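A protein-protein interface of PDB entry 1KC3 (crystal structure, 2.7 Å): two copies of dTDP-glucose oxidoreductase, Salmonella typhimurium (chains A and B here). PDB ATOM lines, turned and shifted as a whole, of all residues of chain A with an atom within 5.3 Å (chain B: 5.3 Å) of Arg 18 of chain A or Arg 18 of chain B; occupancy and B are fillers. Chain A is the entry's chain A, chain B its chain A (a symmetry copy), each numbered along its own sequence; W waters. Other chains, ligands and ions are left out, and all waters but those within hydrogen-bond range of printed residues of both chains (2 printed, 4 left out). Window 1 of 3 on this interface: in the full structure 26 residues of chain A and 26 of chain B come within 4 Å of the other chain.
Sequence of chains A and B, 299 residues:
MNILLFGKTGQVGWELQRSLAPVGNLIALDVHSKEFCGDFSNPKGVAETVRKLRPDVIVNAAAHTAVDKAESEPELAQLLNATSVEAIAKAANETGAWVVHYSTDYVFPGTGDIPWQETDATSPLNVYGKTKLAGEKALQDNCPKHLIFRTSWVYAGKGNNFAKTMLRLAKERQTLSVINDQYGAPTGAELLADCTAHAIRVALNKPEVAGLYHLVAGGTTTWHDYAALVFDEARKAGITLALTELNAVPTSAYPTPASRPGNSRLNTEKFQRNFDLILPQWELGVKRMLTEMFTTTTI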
ATOM      1  N   TRP A  14       8.358  -8.001 -18.683  1.00  0.00           N
ATOM      2  CA  TRP A  14       7.393  -7.022 -18.124  1.00  0.00           C
ATOM      3  C   TRP A  14       8.145  -5.764 -17.764  1.00  0.00           C
ATOM      4  O   TRP A  14       7.659  -4.714 -17.905  1.00  0.00           O
ATOM      5  CB  TRP A  14       6.725  -7.612 -16.858  1.00  0.00           C
ATOM      6  CG  TRP A  14       5.734  -6.747 -16.121  1.00  0.00           C
ATOM      7  CD1 TRP A  14       5.890  -6.176 -14.912  1.00  0.00           C
ATOM      8  CD2 TRP A  14       4.441  -6.412 -16.577  1.00  0.00           C
ATOM      9  NE1 TRP A  14       4.756  -5.476 -14.582  1.00  0.00           N
ATOM     10  CE2 TRP A  14       3.874  -5.567 -15.624  1.00  0.00           C
ATOM     11  CE3 TRP A  14       3.739  -6.663 -17.765  1.00  0.00           C
ATOM     12  CZ2 TRP A  14       2.629  -5.015 -15.782  1.00  0.00           C
ATOM     13  CZ3 TRP A  14       2.531  -6.116 -17.934  1.00  0.00           C
ATOM     14  CH2 TRP A  14       1.952  -5.321 -16.921  1.00  0.00           C
ATOM     15  N   GLU A  15       9.359  -5.895 -17.279  1.00  0.00           N
ATOM     16  CA  GLU A  15      10.159  -4.692 -16.924  1.00  0.00           C
ATOM     17  C   GLU A  15      10.744  -3.918 -18.134  1.00  0.00           C
ATOM     18  O   GLU A  15      11.037  -2.724 -18.043  1.00  0.00           O
ATOM     19  CB  GLU A  15      11.284  -5.044 -15.888  1.00  0.00           C
ATOM     20  CG  GLU A  15      10.705  -5.249 -14.530  1.00  0.00           C
ATOM     21  CD  GLU A  15      10.133  -3.981 -13.990  1.00  0.00           C
ATOM     22  OE1 GLU A  15       8.989  -4.014 -13.677  1.00  0.00           O
ATOM     23  OE2 GLU A  15      10.802  -2.951 -13.893  1.00  0.00           O
ATOM     24  N   LEU A  16      10.979  -4.662 -19.192  1.00  0.00           N
ATOM     25  CA  LEU A  16      11.475  -4.101 -20.438  1.00  0.00           C
ATOM     26  C   LEU A  16      10.363  -3.291 -21.162  1.00  0.00           C
ATOM     27  O   LEU A  16      10.630  -2.228 -21.843  1.00  0.00           O
ATOM     28  CB  LEU A  16      11.987  -5.209 -21.333  1.00  0.00           C
ATOM     29  CG  LEU A  16      13.354  -5.769 -20.948  1.00  0.00           C
ATOM     30  CD1 LEU A  16      13.498  -7.157 -21.568  1.00  0.00           C
ATOM     31  CD2 LEU A  16      14.373  -4.695 -21.442  1.00  0.00           C
ATOM     32  N   GLN A  17       9.136  -3.717 -20.916  1.00  0.00           N
ATOM     33  CA  GLN A  17       7.992  -2.933 -21.367  1.00  0.00           C
ATOM     34  C   GLN A  17       8.045  -1.542 -20.857  1.00  0.00           C
ATOM     35  O   GLN A  17       7.856  -0.643 -21.588  1.00  0.00           O
ATOM     36  CB  GLN A  17       6.598  -3.580 -21.048  1.00  0.00           C
ATOM     37  CG  GLN A  17       6.122  -4.575 -22.104  1.00  0.00           C
ATOM     38  CD  GLN A  17       4.796  -5.121 -21.771  1.00  0.00           C
ATOM     39  OE1 GLN A  17       3.796  -4.613 -22.313  1.00  0.00           O
ATOM     40  NE2 GLN A  17       4.736  -6.188 -20.973  1.00  0.00           N
ATOM     41  N   ARG A  18       8.345  -1.401 -19.572  1.00  0.00           N
ATOM     42  CA  ARG A  18       8.608  -0.067 -18.907  1.00  0.00           C
ATOM     43  C   ARG A  18       9.862   0.595 -19.388  1.00  0.00           C
ATOM     44  O   ARG A  18       9.774   1.729 -19.874  1.00  0.00           O
ATOM     45  CB  ARG A  18       8.710  -0.251 -17.441  1.00  0.00           C
ATOM     46  CG  ARG A  18       8.871   1.003 -16.636  1.00  0.00           C
ATOM     47  CD  ARG A  18       9.349   0.795 -15.268  1.00  0.00           C
ATOM     48  NE  ARG A  18      10.383  -0.252 -15.092  1.00  0.00           N
ATOM     49  CZ  ARG A  18      11.600  -0.159 -15.476  1.00  0.00           C
ATOM     50  NH1 ARG A  18      12.015   0.909 -16.165  1.00  0.00           N
ATOM     51  NH2 ARG A  18      12.435  -1.175 -15.194  1.00  0.00           N
ATOM     52  N   SER A  19      11.011  -0.110 -19.311  1.00  0.00           N
ATOM     53  CA  SER A  19      12.342   0.492 -19.642  1.00  0.00           C
ATOM     54  C   SER A  19      12.623   0.916 -21.066  1.00  0.00           C
ATOM     55  O   SER A  19      13.401   1.902 -21.246  1.00  0.00           O
ATOM     56  CB  SER A  19      13.547  -0.351 -19.221  1.00  0.00           C
ATOM     57  OG  SER A  19      13.643  -1.667 -19.714  1.00  0.00           O
ATOM     58  N   LEU A  20      12.098   0.119 -22.044  1.00  0.00           N
ATOM     59  CA  LEU A  20      12.235   0.424 -23.482  1.00  0.00           C
ATOM     60  C   LEU A  20      11.249   1.458 -23.983  1.00  0.00           C
ATOM     61  O   LEU A  20      11.496   2.153 -24.962  1.00  0.00           O
ATOM     62  CB  LEU A  20      12.126  -0.804 -24.317  1.00  0.00           C
ATOM     63  CG  LEU A  20      13.042  -1.889 -23.832  1.00  0.00           C
ATOM     64  CD1 LEU A  20      12.823  -3.070 -24.697  1.00  0.00           C
ATOM     65  CD2 LEU A  20      14.511  -1.500 -23.932  1.00  0.00           C
ATOM     66  N   ALA A  21      10.154   1.622 -23.280  1.00  0.00           N
ATOM     67  CA  ALA A  21       9.093   2.598 -23.677  1.00  0.00           C
ATOM     68  C   ALA A  21       9.574   3.993 -24.146  1.00  0.00           C
ATOM     69  O   ALA A  21       8.970   4.504 -25.043  1.00  0.00           O
ATOM     70  CB  ALA A  21       7.996   2.748 -22.525  1.00  0.00           C
ATOM     71  N   PRO A  22      10.540   4.633 -23.469  1.00  0.00           N
ATOM     72  CA  PRO A  22      11.102   5.905 -23.940  1.00  0.00           C
ATOM     73  C   PRO A  22      12.331   5.763 -24.880  1.00  0.00           C
ATOM     74  O   PRO A  22      12.696   6.722 -25.618  1.00  0.00           O
ATOM     75  CB  PRO A  22      11.541   6.602 -22.640  1.00  0.00           C
ATOM     76  CG  PRO A  22      11.663   5.484 -21.535  1.00  0.00           C
ATOM     77  CD  PRO A  22      11.127   4.246 -22.159  1.00  0.00           C
ATOM     78  N   GLU A 190      14.251  -5.568 -12.799  1.00  0.00           N
ATOM     79  CA  GLU A 190      14.384  -4.140 -12.879  1.00  0.00           C
ATOM     80  C   GLU A 190      15.745  -3.750 -13.377  1.00  0.00           C
ATOM     81  O   GLU A 190      15.875  -2.992 -14.332  1.00  0.00           O
ATOM     82  CB  GLU A 190      14.174  -3.499 -11.473  1.00  0.00           C
ATOM     83  CG  GLU A 190      12.709  -3.412 -11.020  1.00  0.00           C
ATOM     84  CD  GLU A 190      12.581  -2.911  -9.540  1.00  0.00           C
ATOM     85  OE1 GLU A 190      13.528  -3.046  -8.785  1.00  0.00           O
ATOM     86  OE2 GLU A 190      11.516  -2.383  -9.122  1.00  0.00           O
ATOM     87  N   ALA A 193      16.386  -4.910 -16.969  1.00  0.00           N
ATOM     88  CA  ALA A 193      15.683  -4.096 -17.918  1.00  0.00           C
ATOM     89  C   ALA A 193      16.237  -2.671 -18.051  1.00  0.00           C
ATOM     90  O   ALA A 193      16.187  -2.077 -19.105  1.00  0.00           O
ATOM     91  CB  ALA A 193      14.148  -4.049 -17.593  1.00  0.00           C
ATOM     92  N   ASP A 194      16.755  -2.136 -16.966  1.00  0.00           N
ATOM     93  CA  ASP A 194      17.213  -0.735 -16.917  1.00  0.00           C
ATOM     94  C   ASP A 194      18.552  -0.561 -17.610  1.00  0.00           C
ATOM     95  O   ASP A 194      18.747   0.372 -18.433  1.00  0.00           O
ATOM     96  CB  ASP A 194      17.215  -0.249 -15.483  1.00  0.00           C
ATOM     97  CG  ASP A 194      15.849   0.110 -15.023  1.00  0.00           C
ATOM     98  OD1 ASP A 194      15.727   0.292 -13.735  1.00  0.00           O
ATOM     99  OD2 ASP A 194      14.831   0.151 -15.920  1.00  0.00           O
ATOM    100  N   ARG A 288      14.014  -3.999  -2.223  1.00  0.00           N
ATOM    101  CA  ARG A 288      13.041  -3.248  -3.023  1.00  0.00           C
ATOM    102  C   ARG A 288      11.784  -4.106  -3.498  1.00  0.00           C
ATOM    103  O   ARG A 288      10.669  -3.667  -3.295  1.00  0.00           O
ATOM    104  CB  ARG A 288      13.708  -2.610  -4.208  1.00  0.00           C
ATOM    105  CG  ARG A 288      12.895  -1.647  -4.820  1.00  0.00           C
ATOM    106  CD  ARG A 288      13.491  -1.124  -6.062  1.00  0.00           C
ATOM    107  NE  ARG A 288      12.430  -0.635  -6.943  1.00  0.00           N
ATOM    108  CZ  ARG A 288      11.839   0.555  -6.907  1.00  0.00           C
ATOM    109  NH1 ARG A 288      12.119   1.461  -6.009  1.00  0.00           N
ATOM    110  NH2 ARG A 288      10.822   0.755  -7.723  1.00  0.00           N
ATOM    111  N   TRP B  14      10.541   6.993  -5.371  1.00  0.00           N
ATOM    112  CA  TRP B  14      10.638   5.518  -5.230  1.00  0.00           C
ATOM    113  C   TRP B  14      11.079   4.942  -6.553  1.00  0.00           C
ATOM    114  O   TRP B  14      11.795   4.023  -6.597  1.00  0.00           O
ATOM    115  CB  TRP B  14       9.256   4.939  -4.842  1.00  0.00           C
ATOM    116  CG  TRP B  14       9.141   3.444  -4.688  1.00  0.00           C
ATOM    117  CD1 TRP B  14       8.486   2.587  -5.494  1.00  0.00           C
ATOM    118  CD2 TRP B  14       9.691   2.684  -3.632  1.00  0.00           C
ATOM    119  NE1 TRP B  14       8.607   1.309  -5.007  1.00  0.00           N
ATOM    120  CE2 TRP B  14       9.394   1.347  -3.889  1.00  0.00           C
ATOM    121  CE3 TRP B  14      10.507   3.001  -2.537  1.00  0.00           C
ATOM    122  CZ2 TRP B  14       9.827   0.331  -3.076  1.00  0.00           C
ATOM    123  CZ3 TRP B  14      10.947   2.015  -1.748  1.00  0.00           C
ATOM    124  CH2 TRP B  14      10.571   0.676  -1.991  1.00  0.00           C
ATOM    125  N   GLU B  15      10.623   5.504  -7.648  1.00  0.00           N
ATOM    126  CA  GLU B  15      11.038   4.995  -8.983  1.00  0.00           C
ATOM    127  C   GLU B  15      12.479   5.376  -9.407  1.00  0.00           C
ATOM    128  O   GLU B  15      13.098   4.703 -10.233  1.00  0.00           O
ATOM    129  CB  GLU B  15      10.002   5.398 -10.091  1.00  0.00           C
ATOM    130  CG  GLU B  15       8.768   4.569  -9.987  1.00  0.00           C
ATOM    131  CD  GLU B  15       9.052   3.136 -10.295  1.00  0.00           C
ATOM    132  OE1 GLU B  15       8.764   2.352  -9.453  1.00  0.00           O
ATOM    133  OE2 GLU B  15       9.576   2.787 -11.354  1.00  0.00           O
ATOM    134  N   LEU B  16      12.916   6.504  -8.891  1.00  0.00           N
ATOM    135  CA  LEU B  16      14.263   6.995  -9.132  1.00  0.00           C
ATOM    136  C   LEU B  16      15.309   6.147  -8.354  1.00  0.00           C
ATOM    137  O   LEU B  16      16.482   5.904  -8.834  1.00  0.00           O
ATOM    138  CB  LEU B  16      14.360   8.450  -8.728  1.00  0.00           C
ATOM    139  CG  LEU B  16      13.740   9.436  -9.715  1.00  0.00           C
ATOM    140  CD1 LEU B  16      13.446  10.738  -8.974  1.00  0.00           C
ATOM    141  CD2 LEU B  16      14.776   9.534 -10.878  1.00  0.00           C
ATOM    142  N   GLN B  17      14.847   5.609  -7.238  1.00  0.00           N
ATOM    143  CA  GLN B  17      15.654   4.633  -6.515  1.00  0.00           C
ATOM    144  C   GLN B  17      16.041   3.493  -7.380  1.00  0.00           C
ATOM    145  O   GLN B  17      17.154   3.121  -7.394  1.00  0.00           O
ATOM    146  CB  GLN B  17      15.003   4.113  -5.185  1.00  0.00           C
ATOM    147  CG  GLN B  17      15.284   4.997  -3.972  1.00  0.00           C
ATOM    148  CD  GLN B  17      14.681   4.443  -2.749  1.00  0.00           C
ATOM    149  OE1 GLN B  17      15.404   3.777  -1.984  1.00  0.00           O
ATOM    150  NE2 GLN B  17      13.412   4.753  -2.476  1.00  0.00           N
ATOM    151  N   ARG B  18      15.077   2.973  -8.130  1.00  0.00           N
ATOM    152  CA  ARG B  18      15.308   1.921  -9.193  1.00  0.00           C
ATOM    153  C   ARG B  18      16.098   2.425 -10.360  1.00  0.00           C
ATOM    154  O   ARG B  18      17.149   1.840 -10.650  1.00  0.00           O
ATOM    155  CB  ARG B  18      14.006   1.421  -9.691  1.00  0.00           C
ATOM    156  CG  ARG B  18      14.076   0.298 -10.682  1.00  0.00           C
ATOM    157  CD  ARG B  18      12.844   0.076 -11.442  1.00  0.00           C
ATOM    158  NE  ARG B  18      12.108   1.294 -11.859  1.00  0.00           N
ATOM    159  CZ  ARG B  18      12.491   2.112 -12.765  1.00  0.00           C
ATOM    160  NH1 ARG B  18      13.675   1.957 -13.366  1.00  0.00           N
ATOM    161  NH2 ARG B  18      11.685   3.145 -13.069  1.00  0.00           N
ATOM    162  N   SER B  19      15.642   3.526 -10.996  1.00  0.00           N
ATOM    163  CA  SER B  19      16.276   4.045 -12.250  1.00  0.00           C
ATOM    164  C   SER B  19      17.687   4.586 -12.190  1.00  0.00           C
ATOM    165  O   SER B  19      18.413   4.457 -13.223  1.00  0.00           O
ATOM    166  CB  SER B  19      15.461   5.109 -12.986  1.00  0.00           C
ATOM    167  OG  SER B  19      15.105   6.277 -12.283  1.00  0.00           O
ATOM    168  N   LEU B  20      18.019   5.272 -11.057  1.00  0.00           N
ATOM    169  CA  LEU B  20      19.371   5.817 -10.819  1.00  0.00           C
ATOM    170  C   LEU B  20      20.365   4.787 -10.325  1.00  0.00           C
ATOM    171  O   LEU B  20      21.569   4.920 -10.516  1.00  0.00           O
ATOM    172  CB  LEU B  20      19.342   6.966  -9.873  1.00  0.00           C
ATOM    173  CG  LEU B  20      18.331   7.997 -10.282  1.00  0.00           C
ATOM    174  CD1 LEU B  20      18.352   9.065  -9.257  1.00  0.00           C
ATOM    175  CD2 LEU B  20      18.655   8.631 -11.627  1.00  0.00           C
ATOM    176  N   ALA B  21      19.872   3.717  -9.747  1.00  0.00           N
ATOM    177  CA  ALA B  21      20.747   2.636  -9.200  1.00  0.00           C
ATOM    178  C   ALA B  21      21.941   2.196 -10.083  1.00  0.00           C
ATOM    179  O   ALA B  21      22.961   1.922  -9.521  1.00  0.00           O
ATOM    180  CB  ALA B  21      19.879   1.365  -8.768  1.00  0.00           C
ATOM    181  N   PRO B  22      21.769   2.009 -11.400  1.00  0.00           N
ATOM    182  CA  PRO B  22      22.896   1.700 -12.291  1.00  0.00           C
ATOM    183  C   PRO B  22      23.597   2.943 -12.906  1.00  0.00           C
ATOM    184  O   PRO B  22      24.757   2.854 -13.399  1.00  0.00           O
ATOM    185  CB  PRO B  22      22.242   0.881 -13.418  1.00  0.00           C
ATOM    186  CG  PRO B  22      20.696   1.186 -13.374  1.00  0.00           C
ATOM    187  CD  PRO B  22      20.484   1.997 -12.147  1.00  0.00           C
ATOM    188  N   GLU B 190       7.215   6.024 -13.324  1.00  0.00           N
ATOM    189  CA  GLU B 190       8.106   5.181 -14.071  1.00  0.00           C
ATOM    190  C   GLU B 190       8.754   5.936 -15.193  1.00  0.00           C
ATOM    191  O   GLU B 190       9.973   5.948 -15.327  1.00  0.00           O
ATOM    192  CB  GLU B 190       7.325   3.975 -14.679  1.00  0.00           C
ATOM    193  CG  GLU B 190       6.988   2.860 -13.677  1.00  0.00           C
ATOM    194  CD  GLU B 190       6.067   1.760 -14.312  1.00  0.00           C
ATOM    195  OE1 GLU B 190       5.385   2.046 -15.280  1.00  0.00           O
ATOM    196  OE2 GLU B 190       6.018   0.596 -13.832  1.00  0.00           O
ATOM    197  N   ALA B 193      11.025   8.757 -13.949  1.00  0.00           N
ATOM    198  CA  ALA B 193      12.261   8.247 -13.430  1.00  0.00           C
ATOM    199  C   ALA B 193      13.200   7.674 -14.500  1.00  0.00           C
ATOM    200  O   ALA B 193      14.402   7.737 -14.376  1.00  0.00           O
ATOM    201  CB  ALA B 193      12.004   7.179 -12.310  1.00  0.00           C
ATOM    202  N   ASP B 194      12.628   7.109 -15.544  1.00  0.00           N
ATOM    203  CA  ASP B 194      13.403   6.411 -16.586  1.00  0.00           C
ATOM    204  C   ASP B 194      14.086   7.390 -17.524  1.00  0.00           C
ATOM    205  O   ASP B 194      15.299   7.261 -17.836  1.00  0.00           O
ATOM    206  CB  ASP B 194      12.513   5.419 -17.305  1.00  0.00           C
ATOM    207  CG  ASP B 194      12.328   4.175 -16.513  1.00  0.00           C
ATOM    208  OD1 ASP B 194      11.380   3.383 -16.939  1.00  0.00           O
ATOM    209  OD2 ASP B 194      13.072   3.977 -15.395  1.00  0.00           O
ATOM    210  N   ARG B 288      -0.516  -0.091 -17.475  1.00  0.00           N
ATOM    211  CA  ARG B 288       0.559  -0.783 -16.758  1.00  0.00           C
ATOM    212  C   ARG B 288       0.436  -0.712 -15.169  1.00  0.00           C
ATOM    213  O   ARG B 288       0.510  -1.745 -14.532  1.00  0.00           O
ATOM    214  CB  ARG B 288       1.903  -0.273 -17.194  1.00  0.00           C
ATOM    215  CG  ARG B 288       2.948  -1.104 -16.769  1.00  0.00           C
ATOM    216  CD  ARG B 288       4.271  -0.532 -17.075  1.00  0.00           C
ATOM    217  NE  ARG B 288       5.260  -1.063 -16.136  1.00  0.00           N
ATOM    218  CZ  ARG B 288       5.911  -2.219 -16.220  1.00  0.00           C
ATOM    219  NH1 ARG B 288       5.704  -3.083 -17.178  1.00  0.00           N
ATOM    220  NH2 ARG B 288       6.680  -2.560 -15.204  1.00  0.00           N
HETATM  221  O   HOH W   1      17.457  -0.581 -11.570  1.00  0.00           O
HETATM  222  O   HOH W   2       9.130   3.958 -18.684  1.00  0.00           O
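The guanidinium group of Arg 288 of chain A lies within hydrogen-bond range of the backbone carbonyl oxygen of Trp 14 of chain B, at 2.6 Å.
The guanidinium group (NH1) of Arg 18 of chain A lies within salt-bridge range of the side-chain carboxylate (OD1) of Asp 194 of chain B.
The side-chain carboxylate of Glu 15 of chain A is in salt-bridge range of the guanidinium group of Arg 288 of chain B (3.1 Å).
The guanidinium group of Arg 18 of chain B lies within salt-bridge range of the side-chain carboxylate of Asp 194 of chain A (2.7 Å).
The guanidinium group (NH1) of Arg 18 of chain B sits close to the guanidinium group (NH1) of Arg 18 of chain A, 3.4 Å away.
O of Trp 14 of chain A lies within hydrogen-bond range of NH1 of Arg 288 of chain B (2.6 Å).
The guanidinium group (NH2) of Arg 288 of chain A is in salt-bridge range of the side-chain carboxylate (OE1) of Glu 15 of chain B (3.1 Å).
OE2 of Glu 15 of chain B lies within salt-bridge range of NH2 of Arg 18 of chain B (2.7 Å).
The guanidinium group (NH2) of Arg 18 of chain A lies within salt-bridge range of the side-chain carboxylate (OD2) of Asp 194 of chain A (2.8 Å).
O of Glu 15 of chain A sits at hydrogen-bond distance from OG of Ser 19 of chain A (3.3 Å).
The side-chain carboxylate (OE2) of Glu 190 of chain B lies within salt-bridge range of the guanidinium group (NE) of Arg 288 of chain B (2.9 Å).
The side-chain carboxylate (OE2) of Glu 15 of chain A is in salt-bridge range of the guanidinium group (NH2) of Arg 18 of chain A.
The side-chain carboxylate (OD2) of Asp 194 of chain B is in salt-bridge range of the guanidinium group (NH2) of Arg 18 of chain B (2.8 Å).
Arg 18 of chain A touches Glu 190 of chain B (CD to CG, 3.5 Å).
Arg 18 of chain A touches Arg 288 of chain B (CB to CZ, 3.6 Å).
CG of Glu 190 of chain A touches CD of Arg 18 of chain B (3.5 Å).
CZ of Arg 288 of chain A touches CB of Arg 18 of chain B (3.6 Å).
Of the printed residues of chain B, Glu 15 of chain A touches Arg 288.
Leu 16 of chain A touches none of the printed residues of chain B.
Of the printed residues of chain B, Arg 18 of chain A touches Arg 18 (3.4 Å), Glu 190 (3.5 Å), Asp 194 (2.7 Å) and Arg 288 (3.6 Å).
Ser 19 of chain A touches none of the printed residues of chain B.
Of the printed residues of chain B, Glu 190 of chain A touches Arg 18 (3.5 Å).
Of the printed residues of chain B, Asp 194 of chain A touches Arg 18 (2.7 Å).
Of the printed residues of chain A, Glu 15 of chain B touches Arg 288 (3.1 Å).
Arg 18 of chain B touches just these residues of chain A: Arg 18 (3.4 Å), Glu 190 (3.5 Å), Asp 194 (2.7 Å) and Arg 288 (3.6 Å).
Of the 13 printed residues of chain B, 6 touch a printed residue of chain A.
Printed residues of chain B that touch a printed residue of chain A: Trp 14, Glu 15, Arg 18, Glu 190, Asp 194 and Arg 288.
Among the printed residues, 11 pairs touch across the chains.
Among the printed residues, Asp or Glu carboxylates within 4 Å of a Lys or Arg side-chain nitrogen of the other chain: Glu 15 of chain A with Arg 288 of chain B, Arg 18 of chain A with Asp 194 of chain B, Asp 194 of chain A with Arg 18 of chain B and Arg 288 of chain A with Glu 15 of chain B.
Glu 15 of chain A touches Arg 288 of chain B, and with the chains exchanged Arg 288 of chain A touches Glu 15 of chain B.
Arg 18 of chain A touches its own counterpart, Arg 18 of chain B.
Arg 18 of chain A touches Glu 190 of chain B, and with the chains exchanged Glu 190 of chain A touches Arg 18 of chain B.
Arg 18 of chain A touches Arg 288 of chain B, and with the chains exchanged Arg 288 of chain A touches Arg 18 of chain B.
Positions printed for both chains: 14, 15, 16, 17, 18, 19, 20, 21, 22, 190, 193, 194 and 288.
Water W2 bridges O of Arg 18 of chain A (2.6 Å) and OD1 of Asp 194 of chain B (2.9 Å).
Water W1 lies within hydrogen-bond range of the backbone carbonyl oxygen of Arg 18 of chain B and the side-chain carboxylate of Asp 194 of chain A.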
